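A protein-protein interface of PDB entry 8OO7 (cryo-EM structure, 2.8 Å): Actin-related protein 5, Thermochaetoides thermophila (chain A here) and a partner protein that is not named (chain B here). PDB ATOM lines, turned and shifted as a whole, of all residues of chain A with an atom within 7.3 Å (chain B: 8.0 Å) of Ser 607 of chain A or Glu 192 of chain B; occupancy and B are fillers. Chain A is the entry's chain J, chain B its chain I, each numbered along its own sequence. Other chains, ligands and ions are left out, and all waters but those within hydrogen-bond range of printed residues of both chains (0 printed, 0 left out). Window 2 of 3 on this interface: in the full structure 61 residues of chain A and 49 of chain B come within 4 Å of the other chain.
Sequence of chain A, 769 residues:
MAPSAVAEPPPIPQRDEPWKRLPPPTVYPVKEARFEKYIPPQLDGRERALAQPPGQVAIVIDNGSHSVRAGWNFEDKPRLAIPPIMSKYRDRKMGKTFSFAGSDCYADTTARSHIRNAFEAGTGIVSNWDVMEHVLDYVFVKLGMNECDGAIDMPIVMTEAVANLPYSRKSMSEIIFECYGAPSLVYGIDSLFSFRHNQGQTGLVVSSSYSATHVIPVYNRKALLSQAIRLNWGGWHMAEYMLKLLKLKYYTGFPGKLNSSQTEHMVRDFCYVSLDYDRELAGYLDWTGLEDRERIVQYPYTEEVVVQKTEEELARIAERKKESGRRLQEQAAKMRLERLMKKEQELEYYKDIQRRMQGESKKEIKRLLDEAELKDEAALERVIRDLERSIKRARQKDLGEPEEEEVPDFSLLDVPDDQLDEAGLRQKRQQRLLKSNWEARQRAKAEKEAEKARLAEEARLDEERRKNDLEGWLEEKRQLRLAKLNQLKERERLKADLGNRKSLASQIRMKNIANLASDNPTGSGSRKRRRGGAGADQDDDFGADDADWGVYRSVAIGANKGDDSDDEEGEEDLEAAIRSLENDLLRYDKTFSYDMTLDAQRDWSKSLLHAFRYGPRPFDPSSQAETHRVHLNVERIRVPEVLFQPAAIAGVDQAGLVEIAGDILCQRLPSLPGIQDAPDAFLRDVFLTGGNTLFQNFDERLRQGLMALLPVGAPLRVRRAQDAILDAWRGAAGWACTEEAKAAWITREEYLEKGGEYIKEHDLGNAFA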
ATOM      1  N   LEU A 285     -12.350   2.081  30.584  1.00  0.00           N
ATOM      2  CA  LEU A 285     -12.443   0.661  30.903  1.00  0.00           C
ATOM      3  C   LEU A 285     -11.727  -0.236  29.901  1.00  0.00           C
ATOM      4  O   LEU A 285     -11.787  -1.461  30.045  1.00  0.00           O
ATOM      5  CB  LEU A 285     -13.909   0.236  31.023  1.00  0.00           C
ATOM      6  CG  LEU A 285     -14.674   0.861  32.193  1.00  0.00           C
ATOM      7  CD1 LEU A 285     -16.113   0.372  32.235  1.00  0.00           C
ATOM      8  CD2 LEU A 285     -13.965   0.570  33.501  1.00  0.00           C
ATOM      9  N   TRP A 287      -9.037  -2.519  28.284  1.00  0.00           N
ATOM     10  CA  TRP A 287      -8.420  -3.520  29.154  1.00  0.00           C
ATOM     11  C   TRP A 287      -6.930  -3.277  29.376  1.00  0.00           C
ATOM     12  O   TRP A 287      -6.417  -3.548  30.468  1.00  0.00           O
ATOM     13  CB  TRP A 287      -8.651  -4.924  28.595  1.00  0.00           C
ATOM     14  CG  TRP A 287      -9.923  -5.533  29.084  1.00  0.00           C
ATOM     15  CD1 TRP A 287     -11.182  -5.260  28.646  1.00  0.00           C
ATOM     16  CD2 TRP A 287     -10.063  -6.488  30.141  1.00  0.00           C
ATOM     17  NE1 TRP A 287     -12.099  -6.003  29.348  1.00  0.00           N
ATOM     18  CE2 TRP A 287     -11.436  -6.763  30.275  1.00  0.00           C
ATOM     19  CE3 TRP A 287      -9.160  -7.145  30.981  1.00  0.00           C
ATOM     20  CZ2 TRP A 287     -11.928  -7.664  31.213  1.00  0.00           C
ATOM     21  CZ3 TRP A 287      -9.649  -8.039  31.910  1.00  0.00           C
ATOM     22  CH2 TRP A 287     -11.020  -8.290  32.019  1.00  0.00           C
ATOM     23  N   ALA A 600     -13.759 -18.283  24.156  1.00  0.00           N
ATOM     24  CA  ALA A 600     -13.287 -16.919  24.362  1.00  0.00           C
ATOM     25  C   ALA A 600     -14.438 -15.920  24.335  1.00  0.00           C
ATOM     26  O   ALA A 600     -14.474 -14.984  25.141  1.00  0.00           O
ATOM     27  CB  ALA A 600     -12.243 -16.561  23.308  1.00  0.00           C
ATOM     28  N   GLN A 601     -15.394 -16.106  23.421  1.00  0.00           N
ATOM     29  CA  GLN A 601     -16.541 -15.205  23.336  1.00  0.00           C
ATOM     30  C   GLN A 601     -17.406 -15.210  24.590  1.00  0.00           C
ATOM     31  O   GLN A 601     -18.308 -14.372  24.700  1.00  0.00           O
ATOM     32  CB  GLN A 601     -17.405 -15.572  22.126  1.00  0.00           C
ATOM     33  N   ARG A 602     -17.161 -16.120  25.530  1.00  0.00           N
ATOM     34  CA  ARG A 602     -17.876 -16.146  26.796  1.00  0.00           C
ATOM     35  C   ARG A 602     -16.945 -15.970  27.985  1.00  0.00           C
ATOM     36  O   ARG A 602     -17.406 -16.013  29.132  1.00  0.00           O
ATOM     37  CB  ARG A 602     -18.667 -17.455  26.927  1.00  0.00           C
ATOM     38  N   ASP A 603     -15.652 -15.775  27.743  1.00  0.00           N
ATOM     39  CA  ASP A 603     -14.680 -15.592  28.811  1.00  0.00           C
ATOM     40  C   ASP A 603     -14.885 -14.247  29.503  1.00  0.00           C
ATOM     41  O   ASP A 603     -15.162 -13.232  28.857  1.00  0.00           O
ATOM     42  CB  ASP A 603     -13.260 -15.697  28.249  1.00  0.00           C
ATOM     43  CG  ASP A 603     -12.188 -15.717  29.330  1.00  0.00           C
ATOM     44  OD1 ASP A 603     -12.481 -15.388  30.498  1.00  0.00           O
ATOM     45  OD2 ASP A 603     -11.036 -16.065  29.004  1.00  0.00           O
ATOM     46  N   TRP A 604     -14.769 -14.257  30.836  1.00  0.00           N
ATOM     47  CA  TRP A 604     -14.748 -13.016  31.606  1.00  0.00           C
ATOM     48  C   TRP A 604     -13.703 -12.038  31.083  1.00  0.00           C
ATOM     49  O   TRP A 604     -13.915 -10.821  31.121  1.00  0.00           O
ATOM     50  CB  TRP A 604     -14.483 -13.324  33.084  1.00  0.00           C
ATOM     51  CG  TRP A 604     -13.138 -13.946  33.340  1.00  0.00           C
ATOM     52  CD1 TRP A 604     -12.865 -15.276  33.465  1.00  0.00           C
ATOM     53  CD2 TRP A 604     -11.890 -13.264  33.520  1.00  0.00           C
ATOM     54  NE1 TRP A 604     -11.526 -15.466  33.697  1.00  0.00           N
ATOM     55  CE2 TRP A 604     -10.905 -14.245  33.736  1.00  0.00           C
ATOM     56  CE3 TRP A 604     -11.511 -11.918  33.513  1.00  0.00           C
ATOM     57  CZ2 TRP A 604      -9.567 -13.925  33.943  1.00  0.00           C
ATOM     58  CZ3 TRP A 604     -10.183 -11.603  33.714  1.00  0.00           C
ATOM     59  CH2 TRP A 604      -9.227 -12.601  33.930  1.00  0.00           C
ATOM     60  N   SER A 605     -12.575 -12.552  30.583  1.00  0.00           N
ATOM     61  CA  SER A 605     -11.518 -11.716  30.021  1.00  0.00           C
ATOM     62  C   SER A 605     -11.989 -10.878  28.840  1.00  0.00           C
ATOM     63  O   SER A 605     -11.298  -9.928  28.456  1.00  0.00           O
ATOM     64  CB  SER A 605     -10.335 -12.590  29.596  1.00  0.00           C
ATOM     65  OG  SER A 605      -9.248 -11.799  29.149  1.00  0.00           O
ATOM     66  N   LYS A 606     -13.134 -11.206  28.252  1.00  0.00           N
ATOM     67  CA  LYS A 606     -13.709 -10.433  27.161  1.00  0.00           C
ATOM     68  C   LYS A 606     -14.954  -9.659  27.583  1.00  0.00           C
ATOM     69  O   LYS A 606     -15.690  -9.175  26.716  1.00  0.00           O
ATOM     70  CB  LYS A 606     -14.036 -11.353  25.985  1.00  0.00           C
ATOM     71  CG  LYS A 606     -12.880 -12.246  25.561  1.00  0.00           C
ATOM     72  CD  LYS A 606     -11.647 -11.448  25.178  1.00  0.00           C
ATOM     73  CE  LYS A 606     -10.483 -12.370  24.854  1.00  0.00           C
ATOM     74  NZ  LYS A 606      -9.239 -11.623  24.525  1.00  0.00           N
ATOM     75  N   SER A 607     -15.214  -9.540  28.883  1.00  0.00           N
ATOM     76  CA  SER A 607     -16.423  -8.904  29.394  1.00  0.00           C
ATOM     77  C   SER A 607     -16.096  -7.550  30.011  1.00  0.00           C
ATOM     78  O   SER A 607     -15.153  -7.425  30.800  1.00  0.00           O
ATOM     79  CB  SER A 607     -17.124  -9.798  30.419  1.00  0.00           C
ATOM     80  OG  SER A 607     -16.418  -9.835  31.643  1.00  0.00           O
ATOM     81  N   LEU A 608     -16.882  -6.542  29.630  1.00  0.00           N
ATOM     82  CA  LEU A 608     -16.716  -5.182  30.131  1.00  0.00           C
ATOM     83  C   LEU A 608     -17.080  -5.068  31.609  1.00  0.00           C
ATOM     84  O   LEU A 608     -16.420  -4.344  32.361  1.00  0.00           O
ATOM     85  CB  LEU A 608     -17.576  -4.230  29.298  1.00  0.00           C
ATOM     86  CG  LEU A 608     -17.608  -2.746  29.660  1.00  0.00           C
ATOM     87  CD1 LEU A 608     -16.220  -2.147  29.575  1.00  0.00           C
ATOM     88  CD2 LEU A 608     -18.574  -2.001  28.756  1.00  0.00           C
ATOM     89  N   LEU A 609     -18.120  -5.781  32.039  1.00  0.00           N
ATOM     90  CA  LEU A 609     -18.582  -5.694  33.422  1.00  0.00           C
ATOM     91  C   LEU A 609     -17.613  -6.319  34.419  1.00  0.00           C
ATOM     92  O   LEU A 609     -17.619  -5.937  35.594  1.00  0.00           O
ATOM     93  CB  LEU A 609     -19.954  -6.345  33.548  1.00  0.00           C
ATOM     94  CG  LEU A 609     -21.059  -5.602  32.807  1.00  0.00           C
ATOM     95  CD1 LEU A 609     -22.322  -6.437  32.767  1.00  0.00           C
ATOM     96  CD2 LEU A 609     -21.308  -4.260  33.458  1.00  0.00           C
ATOM     97  N   HIS A 610     -16.785  -7.274  33.996  1.00  0.00           N
ATOM     98  CA  HIS A 610     -15.702  -7.714  34.873  1.00  0.00           C
ATOM     99  C   HIS A 610     -14.651  -6.626  35.058  1.00  0.00           C
ATOM    100  O   HIS A 610     -14.190  -6.389  36.180  1.00  0.00           O
ATOM    101  CB  HIS A 610     -15.062  -8.986  34.321  1.00  0.00           C
ATOM    102  CG  HIS A 610     -14.008  -9.569  35.207  1.00  0.00           C
ATOM    103  ND1 HIS A 610     -14.262 -10.585  36.104  1.00  0.00           N
ATOM    104  CD2 HIS A 610     -12.690  -9.282  35.326  1.00  0.00           C
ATOM    105  CE1 HIS A 610     -13.146 -10.897  36.739  1.00  0.00           C
ATOM    106  NE2 HIS A 610     -12.179 -10.120  36.286  1.00  0.00           N
ATOM    107  N   ALA A 611     -14.245  -5.969  33.971  1.00  0.00           N
ATOM    108  CA  ALA A 611     -13.310  -4.853  34.075  1.00  0.00           C
ATOM    109  C   ALA A 611     -13.851  -3.761  34.991  1.00  0.00           C
ATOM    110  O   ALA A 611     -13.153  -3.283  35.895  1.00  0.00           O
ATOM    111  CB  ALA A 611     -13.023  -4.287  32.687  1.00  0.00           C
ATOM    112  N   PHE A 612     -15.097  -3.353  34.755  1.00  0.00           N
ATOM    113  CA  PHE A 612     -15.767  -2.348  35.571  1.00  0.00           C
ATOM    114  C   PHE A 612     -15.727  -2.694  37.059  1.00  0.00           C
ATOM    115  O   PHE A 612     -15.389  -1.851  37.896  1.00  0.00           O
ATOM    116  CB  PHE A 612     -17.207  -2.217  35.074  1.00  0.00           C
ATOM    117  CG  PHE A 612     -18.013  -1.171  35.775  1.00  0.00           C
ATOM    118  CD1 PHE A 612     -17.544   0.124  35.884  1.00  0.00           C
ATOM    119  CD2 PHE A 612     -19.258  -1.478  36.291  1.00  0.00           C
ATOM    120  CE1 PHE A 612     -18.295   1.093  36.509  1.00  0.00           C
ATOM    121  CE2 PHE A 612     -20.015  -0.516  36.920  1.00  0.00           C
ATOM    122  CZ  PHE A 612     -19.534   0.773  37.028  1.00  0.00           C
ATOM    123  N   GLY A 615     -11.618  -5.362  37.386  1.00  0.00           N
ATOM    124  CA  GLY A 615     -10.389  -5.009  36.721  1.00  0.00           C
ATOM    125  C   GLY A 615      -9.704  -6.164  36.024  1.00  0.00           C
ATOM    126  O   GLY A 615     -10.303  -7.210  35.758  1.00  0.00           O
ATOM    127  N   THR B 173     -22.482   1.720  33.626  1.00  0.00           N
ATOM    128  CA  THR B 173     -21.039   1.915  33.609  1.00  0.00           C
ATOM    129  C   THR B 173     -20.608   3.370  33.472  1.00  0.00           C
ATOM    130  O   THR B 173     -19.416   3.655  33.618  1.00  0.00           O
ATOM    131  CB  THR B 173     -20.415   1.098  32.470  1.00  0.00           C
ATOM    132  OG1 THR B 173     -21.058   1.431  31.233  1.00  0.00           O
ATOM    133  CG2 THR B 173     -20.559  -0.394  32.737  1.00  0.00           C
ATOM    134  N   TYR B 188     -27.725   2.915  28.165  1.00  0.00           N
ATOM    135  CA  TYR B 188     -26.747   1.839  28.220  1.00  0.00           C
ATOM    136  C   TYR B 188     -25.743   1.939  27.082  1.00  0.00           C
ATOM    137  O   TYR B 188     -26.013   2.518  26.027  1.00  0.00           O
ATOM    138  CB  TYR B 188     -27.452   0.472  28.211  1.00  0.00           C
ATOM    139  CG  TYR B 188     -28.189   0.122  26.938  1.00  0.00           C
ATOM    140  CD1 TYR B 188     -29.510   0.507  26.766  1.00  0.00           C
ATOM    141  CD2 TYR B 188     -27.589  -0.621  25.934  1.00  0.00           C
ATOM    142  CE1 TYR B 188     -30.203   0.192  25.623  1.00  0.00           C
ATOM    143  CE2 TYR B 188     -28.283  -0.944  24.781  1.00  0.00           C
ATOM    144  CZ  TYR B 188     -29.590  -0.535  24.635  1.00  0.00           C
ATOM    145  OH  TYR B 188     -30.294  -0.848  23.499  1.00  0.00           O
ATOM    146  N   HIS B 189     -24.565   1.366  27.332  1.00  0.00           N
ATOM    147  CA  HIS B 189     -23.412   1.504  26.453  1.00  0.00           C
ATOM    148  C   HIS B 189     -23.469   0.545  25.270  1.00  0.00           C
ATOM    149  O   HIS B 189     -23.233   0.949  24.126  1.00  0.00           O
ATOM    150  CB  HIS B 189     -22.131   1.298  27.263  1.00  0.00           C
ATOM    151  CG  HIS B 189     -20.874   1.511  26.484  1.00  0.00           C
ATOM    152  ND1 HIS B 189     -20.546   2.724  25.916  1.00  0.00           N
ATOM    153  CD2 HIS B 189     -19.845   0.675  26.210  1.00  0.00           C
ATOM    154  CE1 HIS B 189     -19.378   2.618  25.308  1.00  0.00           C
ATOM    155  NE2 HIS B 189     -18.932   1.385  25.472  1.00  0.00           N
ATOM    156  N   ASN B 190     -23.789  -0.723  25.520  1.00  0.00           N
ATOM    157  CA  ASN B 190     -23.631  -1.760  24.506  1.00  0.00           C
ATOM    158  C   ASN B 190     -24.568  -2.926  24.813  1.00  0.00           C
ATOM    159  O   ASN B 190     -25.356  -2.888  25.761  1.00  0.00           O
ATOM    160  CB  ASN B 190     -22.161  -2.188  24.390  1.00  0.00           C
ATOM    161  CG  ASN B 190     -21.647  -2.927  25.617  1.00  0.00           C
ATOM    162  OD1 ASN B 190     -22.385  -3.198  26.561  1.00  0.00           O
ATOM    163  ND2 ASN B 190     -20.358  -3.252  25.603  1.00  0.00           N
ATOM    164  N   LYS B 191     -24.488  -3.960  23.970  1.00  0.00           N
ATOM    165  CA  LYS B 191     -25.325  -5.147  24.124  1.00  0.00           C
ATOM    166  C   LYS B 191     -25.034  -5.920  25.406  1.00  0.00           C
ATOM    167  O   LYS B 191     -25.945  -6.539  25.968  1.00  0.00           O
ATOM    168  CB  LYS B 191     -25.169  -6.050  22.897  1.00  0.00           C
ATOM    169  CG  LYS B 191     -23.813  -6.714  22.761  1.00  0.00           C
ATOM    170  CD  LYS B 191     -23.761  -7.627  21.548  1.00  0.00           C
ATOM    171  CE  LYS B 191     -22.431  -8.357  21.465  1.00  0.00           C
ATOM    172  NZ  LYS B 191     -22.402  -9.339  20.349  1.00  0.00           N
ATOM    173  N   GLU B 192     -23.785  -5.914  25.877  1.00  0.00           N
ATOM    174  CA  GLU B 192     -23.473  -6.598  27.130  1.00  0.00           C
ATOM    175  C   GLU B 192     -24.218  -5.979  28.305  1.00  0.00           C
ATOM    176  O   GLU B 192     -24.719  -6.695  29.178  1.00  0.00           O
ATOM    177  CB  GLU B 192     -21.967  -6.587  27.389  1.00  0.00           C
ATOM    178  CG  GLU B 192     -21.591  -7.182  28.734  1.00  0.00           C
ATOM    179  CD  GLU B 192     -20.099  -7.279  28.936  1.00  0.00           C
ATOM    180  OE1 GLU B 192     -19.358  -7.006  27.971  1.00  0.00           O
ATOM    181  OE2 GLU B 192     -19.665  -7.650  30.048  1.00  0.00           O
ATOM    182  N   ILE B 193     -24.292  -4.652  28.347  1.00  0.00           N
ATOM    183  CA  ILE B 193     -24.996  -3.956  29.419  1.00  0.00           C
ATOM    184  C   ILE B 193     -26.510  -4.035  29.240  1.00  0.00           C
ATOM    185  O   ILE B 193     -27.251  -4.101  30.226  1.00  0.00           O
ATOM    186  CB  ILE B 193     -24.488  -2.506  29.489  1.00  0.00           C
ATOM    187  CG1 ILE B 193     -23.072  -2.493  30.061  1.00  0.00           C
ATOM    188  CG2 ILE B 193     -25.409  -1.638  30.330  1.00  0.00           C
ATOM    189  CD1 ILE B 193     -22.230  -1.338  29.601  1.00  0.00           C
ATOM    190  N   PHE B 194     -26.995  -4.052  27.999  1.00  0.00           N
ATOM    191  CA  PHE B 194     -28.413  -4.313  27.757  1.00  0.00           C
ATOM    192  C   PHE B 194     -28.840  -5.674  28.297  1.00  0.00           C
ATOM    193  O   PHE B 194     -29.944  -5.816  28.835  1.00  0.00           O
ATOM    194  CB  PHE B 194     -28.698  -4.218  26.259  1.00  0.00           C
ATOM    195  CG  PHE B 194     -30.146  -4.355  25.901  1.00  0.00           C
ATOM    196  CD1 PHE B 194     -30.985  -3.258  25.924  1.00  0.00           C
ATOM    197  CD2 PHE B 194     -30.659  -5.580  25.513  1.00  0.00           C
ATOM    198  CE1 PHE B 194     -32.315  -3.382  25.585  1.00  0.00           C
ATOM    199  CE2 PHE B 194     -31.987  -5.711  25.172  1.00  0.00           C
ATOM    200  CZ  PHE B 194     -32.817  -4.610  25.207  1.00  0.00           C
ATOM    201  N   ALA B 195     -27.987  -6.687  28.150  1.00  0.00           N
ATOM    202  CA  ALA B 195     -28.282  -8.010  28.695  1.00  0.00           C
ATOM    203  C   ALA B 195     -28.449  -7.979  30.212  1.00  0.00           C
ATOM    204  O   ALA B 195     -29.436  -8.493  30.751  1.00  0.00           O
ATOM    205  CB  ALA B 195     -27.181  -8.993  28.297  1.00  0.00           C
ATOM    206  N   MET B 196     -27.485  -7.383  30.915  1.00  0.00           N
ATOM    207  CA  MET B 196     -27.616  -7.137  32.349  1.00  0.00           C
ATOM    208  C   MET B 196     -28.883  -6.360  32.695  1.00  0.00           C
ATOM    209  O   MET B 196     -29.642  -6.758  33.586  1.00  0.00           O
ATOM    210  CB  MET B 196     -26.385  -6.385  32.844  1.00  0.00           C
ATOM    211  CG  MET B 196     -26.558  -5.715  34.189  1.00  0.00           C
ATOM    212  SD  MET B 196     -25.064  -4.829  34.623  1.00  0.00           S
ATOM    213  CE  MET B 196     -24.857  -3.880  33.118  1.00  0.00           C
ATOM    214  N   ILE B 197     -29.117  -5.239  32.014  1.00  0.00           N
ATOM    215  CA  ILE B 197     -30.225  -4.354  32.370  1.00  0.00           C
ATOM    216  C   ILE B 197     -31.566  -5.075  32.292  1.00  0.00           C
ATOM    217  O   ILE B 197     -32.422  -4.921  33.171  1.00  0.00           O
ATOM    218  CB  ILE B 197     -30.200  -3.098  31.480  1.00  0.00           C
ATOM    219  CG1 ILE B 197     -29.139  -2.118  31.984  1.00  0.00           C
ATOM    220  CG2 ILE B 197     -31.554  -2.447  31.436  1.00  0.00           C
ATOM    221  CD1 ILE B 197     -28.910  -0.946  31.072  1.00  0.00           C
ATOM    222  N   ARG B 198     -31.769  -5.884  31.255  1.00  0.00           N
ATOM    223  CA  ARG B 198     -32.992  -6.673  31.158  1.00  0.00           C
ATOM    224  C   ARG B 198     -33.044  -7.827  32.157  1.00  0.00           C
ATOM    225  O   ARG B 198     -34.138  -8.316  32.457  1.00  0.00           O
ATOM    226  CB  ARG B 198     -33.150  -7.201  29.732  1.00  0.00           C
ATOM    227  CG  ARG B 198     -33.488  -6.122  28.716  1.00  0.00           C
ATOM    228  CD  ARG B 198     -34.905  -5.611  28.904  1.00  0.00           C
ATOM    229  NE  ARG B 198     -35.253  -4.593  27.920  1.00  0.00           N
ATOM    230  CZ  ARG B 198     -35.988  -4.815  26.841  1.00  0.00           C
ATOM    231  NH1 ARG B 198     -36.423  -6.026  26.537  1.00  0.00           N
ATOM    232  NH2 ARG B 198     -36.279  -3.798  26.033  1.00  0.00           N
ATOM    233  N   ASN B 199     -31.905  -8.274  32.678  1.00  0.00           N
ATOM    234  CA  ASN B 199     -31.861  -9.328  33.686  1.00  0.00           C
ATOM    235  C   ASN B 199     -31.914  -8.820  35.124  1.00  0.00           C
ATOM    236  O   ASN B 199     -31.934  -9.641  36.047  1.00  0.00           O
ATOM    237  CB  ASN B 199     -30.598 -10.174  33.503  1.00  0.00           C
ATOM    238  CG  ASN B 199     -30.605 -10.956  32.211  1.00  0.00           C
ATOM    239  OD1 ASN B 199     -31.595 -10.958  31.481  1.00  0.00           O
ATOM    240  ND2 ASN B 199     -29.495 -11.624  31.914  1.00  0.00           N
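The side-chain carboxylate of Glu 192 of chain B is in hydrogen-bond range of the backbone NH of Leu 608 of chain A, at 3.0 Å. OE2 of Glu 192 of chain B lies within hydrogen-bond range of N of Leu 609 of chain A (3.1 Å).
N of Glu 192 of chain B is in hydrogen-bond range of OD1 of Asn 190 of chain B (3.1 Å). OD1 of Asn 190 of chain B lies within hydrogen-bond range of N of Ile 193 of chain B (3.0 Å). OG of Ser 607 of chain A is in hydrogen-bond range of O of Trp 604 of chain A, 2.7 Å away. The side-chain hydroxyl (OG) of Ser 607 of chain A sits close to the backbone NH (N) of His 610 of chain A (3.5 Å).
Printed residues of chain B that touch a printed residue of chain A: Thr 173, His 189, Asn 190, Glu 192, Ile 193 and Met 196. Of the 16 printed residues of chain A, 4 touch a printed residue of chain B. Printed residues of chain A that touch a printed residue of chain B: Ser 607, Leu 608, Leu 609 and Phe 612.
Of chain A, only Ser 607 (3.3 Å), Leu 608 (3.0 Å) and Leu 609 (3.1 Å) come within 4 Å of Glu 192 of chain B. Of the printed residues of chain A, His 189 of chain B touches Leu 608. Of the printed residues of chain A, Ile 193 of chain B touches Leu 608 (3.8 Å). Of the printed residues of chain B, Leu 608 of chain A touches His 189 (3.9 Å), Asn 190 (3.8 Å), Glu 192 (3.0 Å) and Ile 193 (3.8 Å). Of the printed residues of chain B, Phe 612 of chain A touches Thr 173 (3.9 Å). Of the printed residues of chain B, Leu 609 of chain A touches Glu 192 and Met 196. Ile 197 of chain B touches none of the printed residues of chain A. Gln 601 of chain A touches none of the printed residues of chain B. The nearest printed residue of chain B that does not touch Leu 609 of chain A is Thr 173 of chain B (4.003 Å).
CB of Ser 607 of chain A touches OE2 of Glu 192 of chain B, at 3.3 Å. Leu 608 of chain A touches His 189 of chain B (CD2 to CD2, 3.9 Å). ND2 of Asn 190 of chain B touches CD2 of Leu 608 of chain A, at 3.8 Å. CD2 of Leu 608 of chain A touches CD1 of Ile 193 of chain B, 3.8 Å away. CD2 of Leu 609 of chain A touches CE of Met 196 of chain B (3.6 Å). CZ of Phe 612 of chain A touches CA of Thr 173 of chain B, 3.9 Å away.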
